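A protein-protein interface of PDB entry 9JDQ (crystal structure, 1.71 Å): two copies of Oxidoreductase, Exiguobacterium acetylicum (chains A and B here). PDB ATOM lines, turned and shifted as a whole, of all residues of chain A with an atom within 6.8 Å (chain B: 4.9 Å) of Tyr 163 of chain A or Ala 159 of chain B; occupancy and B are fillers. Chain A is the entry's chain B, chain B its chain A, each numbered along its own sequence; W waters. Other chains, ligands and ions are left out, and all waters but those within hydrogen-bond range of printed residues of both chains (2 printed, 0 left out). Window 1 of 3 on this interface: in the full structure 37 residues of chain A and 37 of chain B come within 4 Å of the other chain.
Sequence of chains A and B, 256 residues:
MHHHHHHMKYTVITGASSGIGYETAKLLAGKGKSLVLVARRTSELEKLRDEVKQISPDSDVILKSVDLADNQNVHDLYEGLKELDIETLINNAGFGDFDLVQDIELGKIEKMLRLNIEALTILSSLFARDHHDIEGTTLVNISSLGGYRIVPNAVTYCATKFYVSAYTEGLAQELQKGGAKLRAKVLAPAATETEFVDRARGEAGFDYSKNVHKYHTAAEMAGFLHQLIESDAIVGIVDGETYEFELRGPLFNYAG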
ATOM      1  N   ASN A 116      19.344  23.308  25.199  1.00  0.00           N
ATOM      2  CA  ASN A 116      19.719  24.714  25.337  1.00  0.00           C
ATOM      3  C   ASN A 116      21.239  24.871  25.290  1.00  0.00           C
ATOM      4  O   ASN A 116      21.767  25.908  24.905  1.00  0.00           O
ATOM      5  CB  ASN A 116      19.253  25.309  26.666  1.00  0.00           C
ATOM      6  CG  ASN A 116      17.769  25.577  26.762  1.00  0.00           C
ATOM      7  OD1 ASN A 116      16.959  25.043  25.995  1.00  0.00           O
ATOM      8  ND2 ASN A 116      17.396  26.331  27.790  1.00  0.00           N
ATOM      9  N   ILE A 117      21.939  23.845  25.739  1.00  0.00           N
ATOM     10  CA  ILE A 117      23.402  23.868  25.852  1.00  0.00           C
ATOM     11  C   ILE A 117      24.060  22.981  24.803  1.00  0.00           C
ATOM     12  O   ILE A 117      24.875  23.463  24.002  1.00  0.00           O
ATOM     13  CB  ILE A 117      23.839  23.475  27.266  1.00  0.00           C
ATOM     14  CG1 ILE A 117      23.364  24.522  28.277  1.00  0.00           C
ATOM     15  CG2 ILE A 117      25.350  23.256  27.321  1.00  0.00           C
ATOM     16  CD1 ILE A 117      23.774  24.196  29.691  1.00  0.00           C
ATOM     17  N   GLU A 118      23.605  21.729  24.750  1.00  0.00           N
ATOM     18  CA  GLU A 118      24.391  20.785  23.956  1.00  0.00           C
ATOM     19  C   GLU A 118      24.191  21.007  22.461  1.00  0.00           C
ATOM     20  O   GLU A 118      25.167  21.056  21.696  1.00  0.00           O
ATOM     21  CB  GLU A 118      24.129  19.321  24.327  1.00  0.00           C
ATOM     22  CG  GLU A 118      24.636  19.045  25.727  1.00  0.00           C
ATOM     23  CD  GLU A 118      24.432  17.695  26.343  1.00  0.00           C
ATOM     24  OE1 GLU A 118      23.672  16.905  25.732  1.00  0.00           O
ATOM     25  OE2 GLU A 118      25.070  17.476  27.440  1.00  0.00           O
ATOM     26  N   LEU A 120      23.166  23.531  20.952  1.00  0.00           N
ATOM     27  CA  LEU A 120      23.730  24.824  20.595  1.00  0.00           C
ATOM     28  C   LEU A 120      25.251  24.751  20.442  1.00  0.00           C
ATOM     29  O   LEU A 120      25.804  25.295  19.521  1.00  0.00           O
ATOM     30  CB  LEU A 120      23.299  25.831  21.650  1.00  0.00           C
ATOM     31  CG  LEU A 120      23.797  27.264  21.437  1.00  0.00           C
ATOM     32  CD1 LEU A 120      22.748  28.285  21.837  1.00  0.00           C
ATOM     33  CD2 LEU A 120      25.093  27.502  22.224  1.00  0.00           C
ATOM     34  N   THR A 121      25.914  24.013  21.300  1.00  0.00           N
ATOM     35  CA  THR A 121      27.362  23.884  21.257  1.00  0.00           C
ATOM     36  C   THR A 121      27.792  23.040  20.052  1.00  0.00           C
ATOM     37  O   THR A 121      28.849  23.298  19.454  1.00  0.00           O
ATOM     38  CB  THR A 121      27.853  23.281  22.571  1.00  0.00           C
ATOM     39  OG1 THR A 121      27.527  24.116  23.694  1.00  0.00           O
ATOM     40  CG2 THR A 121      29.367  23.279  22.679  1.00  0.00           C
ATOM     41  N   SER A 143      20.572  33.653  23.681  1.00  0.00           N
ATOM     42  CA  SER A 143      20.577  33.478  25.153  1.00  0.00           C
ATOM     43  C   SER A 143      19.283  34.095  25.704  1.00  0.00           C
ATOM     44  O   SER A 143      18.206  33.803  25.170  1.00  0.00           O
ATOM     45  CB  SER A 143      21.832  34.070  25.802  1.00  0.00           C
ATOM     46  OG  SER A 143      21.842  33.938  27.214  1.00  0.00           O
ATOM     47  N   GLY A 147      20.438  35.171  30.908  1.00  0.00           N
ATOM     48  CA  GLY A 147      21.813  34.695  30.770  1.00  0.00           C
ATOM     49  C   GLY A 147      22.833  35.717  31.247  1.00  0.00           C
ATOM     50  O   GLY A 147      24.036  35.483  31.137  1.00  0.00           O
ATOM     51  N   CYS A 158      18.187  29.847  33.781  1.00  0.00           N
ATOM     52  CA  CYS A 158      19.097  30.981  33.718  1.00  0.00           C
ATOM     53  C   CYS A 158      20.512  30.461  33.545  1.00  0.00           C
ATOM     54  O   CYS A 158      21.237  30.993  32.738  1.00  0.00           O
ATOM     55  CB  CYS A 158      18.993  31.926  34.911  1.00  0.00           C
ATOM     56  SG  CYS A 158      17.456  32.898  34.919  1.00  0.00           S
ATOM     57  N   ALA A 159      20.918  29.467  34.340  1.00  0.00           N
ATOM     58  CA  ALA A 159      22.252  28.891  34.180  1.00  0.00           C
ATOM     59  C   ALA A 159      22.533  28.431  32.739  1.00  0.00           C
ATOM     60  O   ALA A 159      23.606  28.689  32.198  1.00  0.00           O
ATOM     61  CB  ALA A 159      22.423  27.753  35.152  1.00  0.00           C
ATOM     62  N   THR A 160      21.568  27.784  32.070  1.00  0.00           N
ATOM     63  CA  THR A 160      21.775  27.390  30.688  1.00  0.00           C
ATOM     64  C   THR A 160      22.072  28.634  29.841  1.00  0.00           C
ATOM     65  O   THR A 160      22.880  28.537  28.936  1.00  0.00           O
ATOM     66  CB  THR A 160      20.633  26.573  30.073  1.00  0.00           C
ATOM     67  OG1 THR A 160      19.542  27.394  29.689  1.00  0.00           O
ATOM     68  CG2 THR A 160      20.107  25.480  30.992  1.00  0.00           C
ATOM     69  N   LYS A 161      21.488  29.799  30.170  1.00  0.00           N
ATOM     70  CA  LYS A 161      21.649  30.991  29.342  1.00  0.00           C
ATOM     71  C   LYS A 161      22.941  31.725  29.698  1.00  0.00           C
ATOM     72  O   LYS A 161      23.526  32.345  28.834  1.00  0.00           O
ATOM     73  CB  LYS A 161      20.381  31.854  29.378  1.00  0.00           C
ATOM     74  CG  LYS A 161      19.203  31.063  28.845  1.00  0.00           C
ATOM     75  CD  LYS A 161      19.295  30.823  27.348  1.00  0.00           C
ATOM     76  CE  LYS A 161      17.952  30.506  26.662  1.00  0.00           C
ATOM     77  NZ  LYS A 161      18.177  30.106  25.279  1.00  0.00           N
ATOM     78  N   PHE A 162      23.395  31.658  30.959  1.00  0.00           N
ATOM     79  CA  PHE A 162      24.730  32.081  31.300  1.00  0.00           C
ATOM     80  C   PHE A 162      25.754  31.283  30.485  1.00  0.00           C
ATOM     81  O   PHE A 162      26.770  31.856  30.088  1.00  0.00           O
ATOM     82  CB  PHE A 162      24.990  32.019  32.817  1.00  0.00           C
ATOM     83  CG  PHE A 162      24.611  33.272  33.600  1.00  0.00           C
ATOM     84  CD1 PHE A 162      23.283  33.514  33.934  1.00  0.00           C
ATOM     85  CD2 PHE A 162      25.581  34.152  34.096  1.00  0.00           C
ATOM     86  CE1 PHE A 162      22.931  34.694  34.580  1.00  0.00           C
ATOM     87  CE2 PHE A 162      25.222  35.322  34.761  1.00  0.00           C
ATOM     88  CZ  PHE A 162      23.893  35.592  34.986  1.00  0.00           C
ATOM     89  N   TYR A 163      25.530  29.977  30.270  1.00  0.00           N
ATOM     90  CA  TYR A 163      26.378  29.170  29.427  1.00  0.00           C
ATOM     91  C   TYR A 163      26.370  29.725  28.009  1.00  0.00           C
ATOM     92  O   TYR A 163      27.413  29.944  27.414  1.00  0.00           O
ATOM     93  CB  TYR A 163      25.909  27.707  29.306  1.00  0.00           C
ATOM     94  CG  TYR A 163      26.739  26.870  28.364  1.00  0.00           C
ATOM     95  CD1 TYR A 163      26.531  26.917  26.990  1.00  0.00           C
ATOM     96  CD2 TYR A 163      27.841  26.150  28.832  1.00  0.00           C
ATOM     97  CE1 TYR A 163      27.314  26.172  26.115  1.00  0.00           C
ATOM     98  CE2 TYR A 163      28.629  25.415  27.969  1.00  0.00           C
ATOM     99  CZ  TYR A 163      28.381  25.440  26.601  1.00  0.00           C
ATOM    100  OH  TYR A 163      29.179  24.713  25.769  1.00  0.00           O
ATOM    101  N   VAL A 164      25.165  29.984  27.480  1.00  0.00           N
ATOM    102  CA  VAL A 164      25.032  30.476  26.110  1.00  0.00           C
ATOM    103  C   VAL A 164      25.722  31.838  25.951  1.00  0.00           C
ATOM    104  O   VAL A 164      26.486  32.037  25.014  1.00  0.00           O
ATOM    105  CB  VAL A 164      23.584  30.604  25.595  1.00  0.00           C
ATOM    106  CG1 VAL A 164      23.621  31.212  24.207  1.00  0.00           C
ATOM    107  CG2 VAL A 164      22.840  29.276  25.642  1.00  0.00           C
ATOM    108  N   SER A 165      25.531  32.715  26.914  1.00  0.00           N
ATOM    109  CA  SER A 165      26.158  34.038  26.884  1.00  0.00           C
ATOM    110  C   SER A 165      27.685  33.960  26.942  1.00  0.00           C
ATOM    111  O   SER A 165      28.364  34.601  26.121  1.00  0.00           O
ATOM    112  CB  SER A 165      25.591  34.927  27.926  1.00  0.00           C
ATOM    113  OG  SER A 165      24.242  35.237  27.597  1.00  0.00           O
ATOM    114  N   ALA A 166      28.213  33.163  27.882  1.00  0.00           N
ATOM    115  CA  ALA A 166      29.654  33.089  28.064  1.00  0.00           C
ATOM    116  C   ALA A 166      30.277  32.379  26.871  1.00  0.00           C
ATOM    117  O   ALA A 166      31.331  32.797  26.417  1.00  0.00           O
ATOM    118  CB  ALA A 166      30.015  32.418  29.363  1.00  0.00           C
ATOM    119  N   TYR A 167      29.646  31.290  26.423  1.00  0.00           N
ATOM    120  CA  TYR A 167      30.154  30.530  25.300  1.00  0.00           C
ATOM    121  C   TYR A 167      30.226  31.462  24.095  1.00  0.00           C
ATOM    122  O   TYR A 167      31.219  31.495  23.366  1.00  0.00           O
ATOM    123  CB  TYR A 167      29.255  29.315  25.047  1.00  0.00           C
ATOM    124  CG  TYR A 167      29.650  28.477  23.854  1.00  0.00           C
ATOM    125  CD1 TYR A 167      30.692  27.557  23.934  1.00  0.00           C
ATOM    126  CD2 TYR A 167      29.055  28.695  22.608  1.00  0.00           C
ATOM    127  CE1 TYR A 167      31.032  26.784  22.845  1.00  0.00           C
ATOM    128  CE2 TYR A 167      29.406  27.936  21.504  1.00  0.00           C
ATOM    129  CZ  TYR A 167      30.447  27.032  21.615  1.00  0.00           C
ATOM    130  OH  TYR A 167      30.782  26.218  20.569  1.00  0.00           O
ATOM    131  N   THR A 168      29.169  32.227  23.870  1.00  0.00           N
ATOM    132  CA  THR A 168      29.092  32.958  22.625  1.00  0.00           C
ATOM    133  C   THR A 168      30.023  34.172  22.652  1.00  0.00           C
ATOM    134  O   THR A 168      30.677  34.520  21.664  1.00  0.00           O
ATOM    135  CB  THR A 168      27.621  33.307  22.342  1.00  0.00           C
ATOM    136  OG1 THR A 168      26.862  32.082  22.356  1.00  0.00           O
ATOM    137  CG2 THR A 168      27.493  33.987  20.990  1.00  0.00           C
ATOM    138  N   GLU A 169      30.072  34.876  23.774  1.00  0.00           N
ATOM    139  CA  GLU A 169      31.001  35.986  23.874  1.00  0.00           C
ATOM    140  C   GLU A 169      32.429  35.466  23.700  1.00  0.00           C
ATOM    141  O   GLU A 169      33.243  36.107  23.046  1.00  0.00           O
ATOM    142  CB  GLU A 169      30.902  36.751  25.199  1.00  0.00           C
ATOM    143  CG  GLU A 169      29.650  37.604  25.339  1.00  0.00           C
ATOM    144  CD  GLU A 169      29.583  38.448  26.606  1.00  0.00           C
ATOM    145  OE1 GLU A 169      30.564  38.487  27.339  1.00  0.00           O
ATOM    146  OE2 GLU A 169      28.530  39.049  26.833  1.00  0.00           O
ATOM    147  N   PHE A 252      30.648  40.107  29.795  1.00  0.00           N
ATOM    148  CA  PHE A 252      31.458  39.387  30.758  1.00  0.00           C
ATOM    149  C   PHE A 252      32.930  39.757  30.612  1.00  0.00           C
ATOM    150  O   PHE A 252      33.380  40.158  29.543  1.00  0.00           O
ATOM    151  CB  PHE A 252      31.250  37.885  30.561  1.00  0.00           C
ATOM    152  CG  PHE A 252      29.884  37.350  30.950  1.00  0.00           C
ATOM    153  CD1 PHE A 252      29.300  37.671  32.166  1.00  0.00           C
ATOM    154  CD2 PHE A 252      29.201  36.456  30.108  1.00  0.00           C
ATOM    155  CE1 PHE A 252      28.066  37.159  32.522  1.00  0.00           C
ATOM    156  CE2 PHE A 252      27.973  35.952  30.483  1.00  0.00           C
ATOM    157  CZ  PHE A 252      27.417  36.281  31.694  1.00  0.00           C
ATOM    158  N   LEU B 113      30.340  18.369  28.705  1.00  0.00           N
ATOM    159  CA  LEU B 113      29.049  18.931  29.071  1.00  0.00           C
ATOM    160  C   LEU B 113      28.300  17.968  29.992  1.00  0.00           C
ATOM    161  O   LEU B 113      27.685  18.408  30.964  1.00  0.00           O
ATOM    162  CB  LEU B 113      28.222  19.338  27.863  1.00  0.00           C
ATOM    163  CG  LEU B 113      28.865  20.358  26.919  1.00  0.00           C
ATOM    164  CD1 LEU B 113      28.081  20.525  25.649  1.00  0.00           C
ATOM    165  CD2 LEU B 113      29.131  21.689  27.527  1.00  0.00           C
ATOM    166  N   ILE B 117      28.455  19.751  33.703  1.00  0.00           N
ATOM    167  CA  ILE B 117      27.160  20.434  33.769  1.00  0.00           C
ATOM    168  C   ILE B 117      26.077  19.477  34.243  1.00  0.00           C
ATOM    169  O   ILE B 117      25.431  19.717  35.270  1.00  0.00           O
ATOM    170  CB  ILE B 117      26.791  21.072  32.421  1.00  0.00           C
ATOM    171  CG1 ILE B 117      27.740  22.191  32.112  1.00  0.00           C
ATOM    172  CG2 ILE B 117      25.347  21.567  32.427  1.00  0.00           C
ATOM    173  CD1 ILE B 117      27.402  22.934  30.828  1.00  0.00           C
ATOM    174  N   VAL B 155      37.303  28.326  25.720  1.00  0.00           N
ATOM    175  CA  VAL B 155      35.967  28.921  25.726  1.00  0.00           C
ATOM    176  C   VAL B 155      34.915  27.922  26.236  1.00  0.00           C
ATOM    177  O   VAL B 155      34.087  28.317  27.053  1.00  0.00           O
ATOM    178  CB  VAL B 155      35.629  29.508  24.342  1.00  0.00           C
ATOM    179  CG1 VAL B 155      34.178  30.024  24.226  1.00  0.00           C
ATOM    180  CG2 VAL B 155      36.559  30.669  24.046  1.00  0.00           C
ATOM    181  N   THR B 156      34.920  26.677  25.743  1.00  0.00           N
ATOM    182  CA  THR B 156      33.862  25.728  26.074  1.00  0.00           C
ATOM    183  C   THR B 156      33.897  25.413  27.571  1.00  0.00           C
ATOM    184  O   THR B 156      32.904  25.521  28.281  1.00  0.00           O
ATOM    185  CB  THR B 156      33.933  24.447  25.232  1.00  0.00           C
ATOM    186  OG1 THR B 156      33.914  24.863  23.869  1.00  0.00           O
ATOM    187  CG2 THR B 156      32.741  23.544  25.484  1.00  0.00           C
ATOM    188  N   TYR B 157      35.082  25.188  28.088  1.00  0.00           N
ATOM    189  CA  TYR B 157      35.215  24.869  29.490  1.00  0.00           C
ATOM    190  C   TYR B 157      34.765  26.042  30.347  1.00  0.00           C
ATOM    191  O   TYR B 157      34.091  25.867  31.365  1.00  0.00           O
ATOM    192  CB  TYR B 157      36.702  24.562  29.722  1.00  0.00           C
ATOM    193  CG  TYR B 157      37.023  24.516  31.210  1.00  0.00           C
ATOM    194  CD1 TYR B 157      36.712  23.402  31.965  1.00  0.00           C
ATOM    195  CD2 TYR B 157      37.611  25.605  31.851  1.00  0.00           C
ATOM    196  CE1 TYR B 157      37.019  23.337  33.311  1.00  0.00           C
ATOM    197  CE2 TYR B 157      37.900  25.572  33.203  1.00  0.00           C
ATOM    198  CZ  TYR B 157      37.610  24.431  33.927  1.00  0.00           C
ATOM    199  OH  TYR B 157      37.907  24.378  35.240  1.00  0.00           O
ATOM    200  N   CYS B 158      35.227  27.246  29.972  1.00  0.00           N
ATOM    201  CA  CYS B 158      34.804  28.408  30.741  1.00  0.00           C
ATOM    202  C   CYS B 158      33.280  28.489  30.757  1.00  0.00           C
ATOM    203  O   CYS B 158      32.712  28.723  31.811  1.00  0.00           O
ATOM    204  CB  CYS B 158      35.446  29.692  30.255  1.00  0.00           C
ATOM    205  SG  CYS B 158      37.217  29.812  30.634  1.00  0.00           S
ATOM    206  N   ALA B 159      32.627  28.296  29.603  1.00  0.00           N
ATOM    207  CA  ALA B 159      31.162  28.324  29.566  1.00  0.00           C
ATOM    208  C   ALA B 159      30.584  27.291  30.528  1.00  0.00           C
ATOM    209  O   ALA B 159      29.680  27.634  31.266  1.00  0.00           O
ATOM    210  CB  ALA B 159      30.640  28.140  28.176  1.00  0.00           C
ATOM    211  N   THR B 160      31.183  26.087  30.649  1.00  0.00           N
ATOM    212  CA  THR B 160      30.668  25.114  31.595  1.00  0.00           C
ATOM    213  C   THR B 160      30.757  25.689  33.012  1.00  0.00           C
ATOM    214  O   THR B 160      29.879  25.419  33.811  1.00  0.00           O
ATOM    215  CB  THR B 160      31.310  23.720  31.525  1.00  0.00           C
ATOM    216  OG1 THR B 160      32.612  23.755  32.079  1.00  0.00           O
ATOM    217  CG2 THR B 160      31.384  23.130  30.121  1.00  0.00           C
ATOM    218  N   LYS B 161      31.778  26.496  33.310  1.00  0.00           N
ATOM    219  CA  LYS B 161      31.979  27.002  34.659  1.00  0.00           C
ATOM    220  C   LYS B 161      31.141  28.259  34.919  1.00  0.00           C
ATOM    221  O   LYS B 161      30.764  28.480  36.035  1.00  0.00           O
ATOM    222  CB  LYS B 161      33.489  27.144  34.849  1.00  0.00           C
ATOM    223  CG  LYS B 161      34.216  25.828  34.787  1.00  0.00           C
ATOM    224  CD  LYS B 161      33.700  24.756  35.739  1.00  0.00           C
ATOM    225  CE  LYS B 161      34.719  23.651  36.040  1.00  0.00           C
ATOM    226  NZ  LYS B 161      34.301  22.727  37.112  1.00  0.00           N
ATOM    227  N   PHE B 162      30.799  29.037  33.889  1.00  0.00           N
ATOM    228  CA  PHE B 162      29.804  30.072  34.024  1.00  0.00           C
ATOM    229  C   PHE B 162      28.464  29.446  34.420  1.00  0.00           C
ATOM    230  O   PHE B 162      27.713  30.017  35.217  1.00  0.00           O
ATOM    231  CB  PHE B 162      29.718  30.950  32.760  1.00  0.00           C
ATOM    232  CG  PHE B 162      30.635  32.168  32.738  1.00  0.00           C
ATOM    233  CD1 PHE B 162      31.980  32.034  32.431  1.00  0.00           C
ATOM    234  CD2 PHE B 162      30.146  33.457  33.002  1.00  0.00           C
ATOM    235  CE1 PHE B 162      32.826  33.129  32.527  1.00  0.00           C
ATOM    236  CE2 PHE B 162      30.985  34.547  33.023  1.00  0.00           C
ATOM    237  CZ  PHE B 162      32.322  34.390  32.775  1.00  0.00           C
ATOM    238  N   TYR B 163      28.128  28.304  33.817  1.00  0.00           N
ATOM    239  CA  TYR B 163      26.973  27.532  34.209  1.00  0.00           C
ATOM    240  C   TYR B 163      27.022  27.161  35.682  1.00  0.00           C
ATOM    241  O   TYR B 163      26.068  27.411  36.389  1.00  0.00           O
ATOM    242  CB  TYR B 163      26.819  26.233  33.398  1.00  0.00           C
ATOM    243  CG  TYR B 163      25.629  25.412  33.843  1.00  0.00           C
ATOM    244  CD1 TYR B 163      25.701  24.567  34.945  1.00  0.00           C
ATOM    245  CD2 TYR B 163      24.403  25.538  33.191  1.00  0.00           C
ATOM    246  CE1 TYR B 163      24.599  23.814  35.353  1.00  0.00           C
ATOM    247  CE2 TYR B 163      23.301  24.848  33.630  1.00  0.00           C
ATOM    248  CZ  TYR B 163      23.384  23.992  34.719  1.00  0.00           C
ATOM    249  OH  TYR B 163      22.282  23.290  35.076  1.00  0.00           O
HETATM  250  O   HOH W   1      33.617  30.974  27.379  1.00  0.00           O
HETATM  251  O   HOH W   2      32.533  24.393  21.438  1.00  0.00           O
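The side-chain hydroxyl (OG1) of Thr 160 of chain B is in hydrogen-bond range of the backbone carbonyl oxygen (O) of Tyr 157 of chain B, 2.7 Å away. The side-chain amide nitrogen (ND2) of Asn 116 of chain A sits at hydrogen-bond distance from the side-chain hydroxyl (OG1) of Thr 160 of chain A, at 3.1 Å. The backbone carbonyl oxygen (O) of Ile 117 of chain A sits at hydrogen-bond distance from the side-chain hydroxyl (OG1) of Thr 121 of chain A (2.7 Å). OG1 of Thr 121 of chain A lies within hydrogen-bond range of OH of Tyr 163 of chain A, at 2.7 Å. The side-chain carboxylate of Glu 169 of chain A sits at hydrogen-bond distance from the backbone NH of Phe 252 of chain A, at 2.9 Å.
Among the printed residues, merely in contact across the chains: Ile 117 of chain A with Tyr 163 of chain B (3.8 Å), Glu 118 of chain A with Leu 113 of chain B (3.7 Å), Ala 159 of chain A with Tyr 163 of chain B (3.4 Å), Thr 160 of chain A with Tyr 163 of chain B (3.7 Å), Tyr 163 of chain A with Leu 113 of chain B (3.5 Å), Tyr 163 of chain A with Ile 117 of chain B (3.8 Å), Tyr 163 of chain A with Thr 156 of chain B (3.8 Å), Tyr 163 of chain A with Ala 159 of chain B (3.4 Å), Tyr 163 of chain A with Thr 160 of chain B (3.8 Å), Ala 166 of chain A with Phe 162 of chain B (3.4 Å), Tyr 167 of chain A with Val 155 of chain B (3.4 Å), Tyr 167 of chain A with Thr 156 of chain B (3.6 Å), Tyr 167 of chain A with Ala 159 of chain B (3.6 Å) and Phe 252 of chain A with Phe 162 of chain B (3.7 Å).
Of the printed residues of chain B, Ile 117 of chain A touches Tyr 163 (3.8 Å). Lys 161 of chain A touches none of the printed residues of chain B. Of chain B, only Leu 113, Ile 117, Thr 156, Ala 159 and Thr 160 come within 4 Å of Tyr 163 of chain A. Of the printed residues of chain B, Tyr 167 of chain A touches Val 155, Thr 156 and Ala 159. Of the printed residues of chain A, Thr 156 of chain B touches Tyr 163 and Tyr 167. Of chain A, only Tyr 163 and Tyr 167 come within 4 Å of Ala 159 of chain B. Lys 161 of chain B touches none of the printed residues of chain A. Printed residues of chain A within 4 Å of Tyr 163 of chain B: Ile 117, Ala 159 and Thr 160. The nearest printed residue of chain B that does not touch Thr 160 of chain A is Ile 117 of chain B (6.7 Å).
Of the 11 printed residues of chain B, 8 touch a printed residue of chain A. Hydrophobic or aromatic side chains of chain B that line the printed part of chain A: Leu 113, Ile 117, Val 155, Ala 159, Phe 162 and Tyr 163. Of the 20 printed residues of chain A, 8 touch a printed residue of chain B. Among the printed residues, no Asp or Glu carboxylate lies within 4 Å of a Lys or Arg side-chain nitrogen of the other chain.
Ile 117 of chain A touches Tyr 163 of chain B, and with the chains exchanged Tyr 163 of chain A touches Ile 117 of chain B. Ala 159 of chain A touches Tyr 163 of chain B, and with the chains exchanged Tyr 163 of chain A touches Ala 159 of chain B. Thr 160 of chain A touches Tyr 163 of chain B, and with the chains exchanged Tyr 163 of chain A touches Thr 160 of chain B. 7 positions are printed for both chains. Of the 14 pairs that touch across the chains among the printed residues, 6 have their exchanged pair printed and touching as well.
Water W2 lies within hydrogen-bond range of OH of Tyr 167 of chain A (2.7 Å) and OG1 of Thr 156 of chain B (2.8 Å). Water W1 lies within hydrogen-bond range of the backbone carbonyl oxygen of Val 155 of chain B and the backbone carbonyl oxygen of Ala 166 of chain A.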
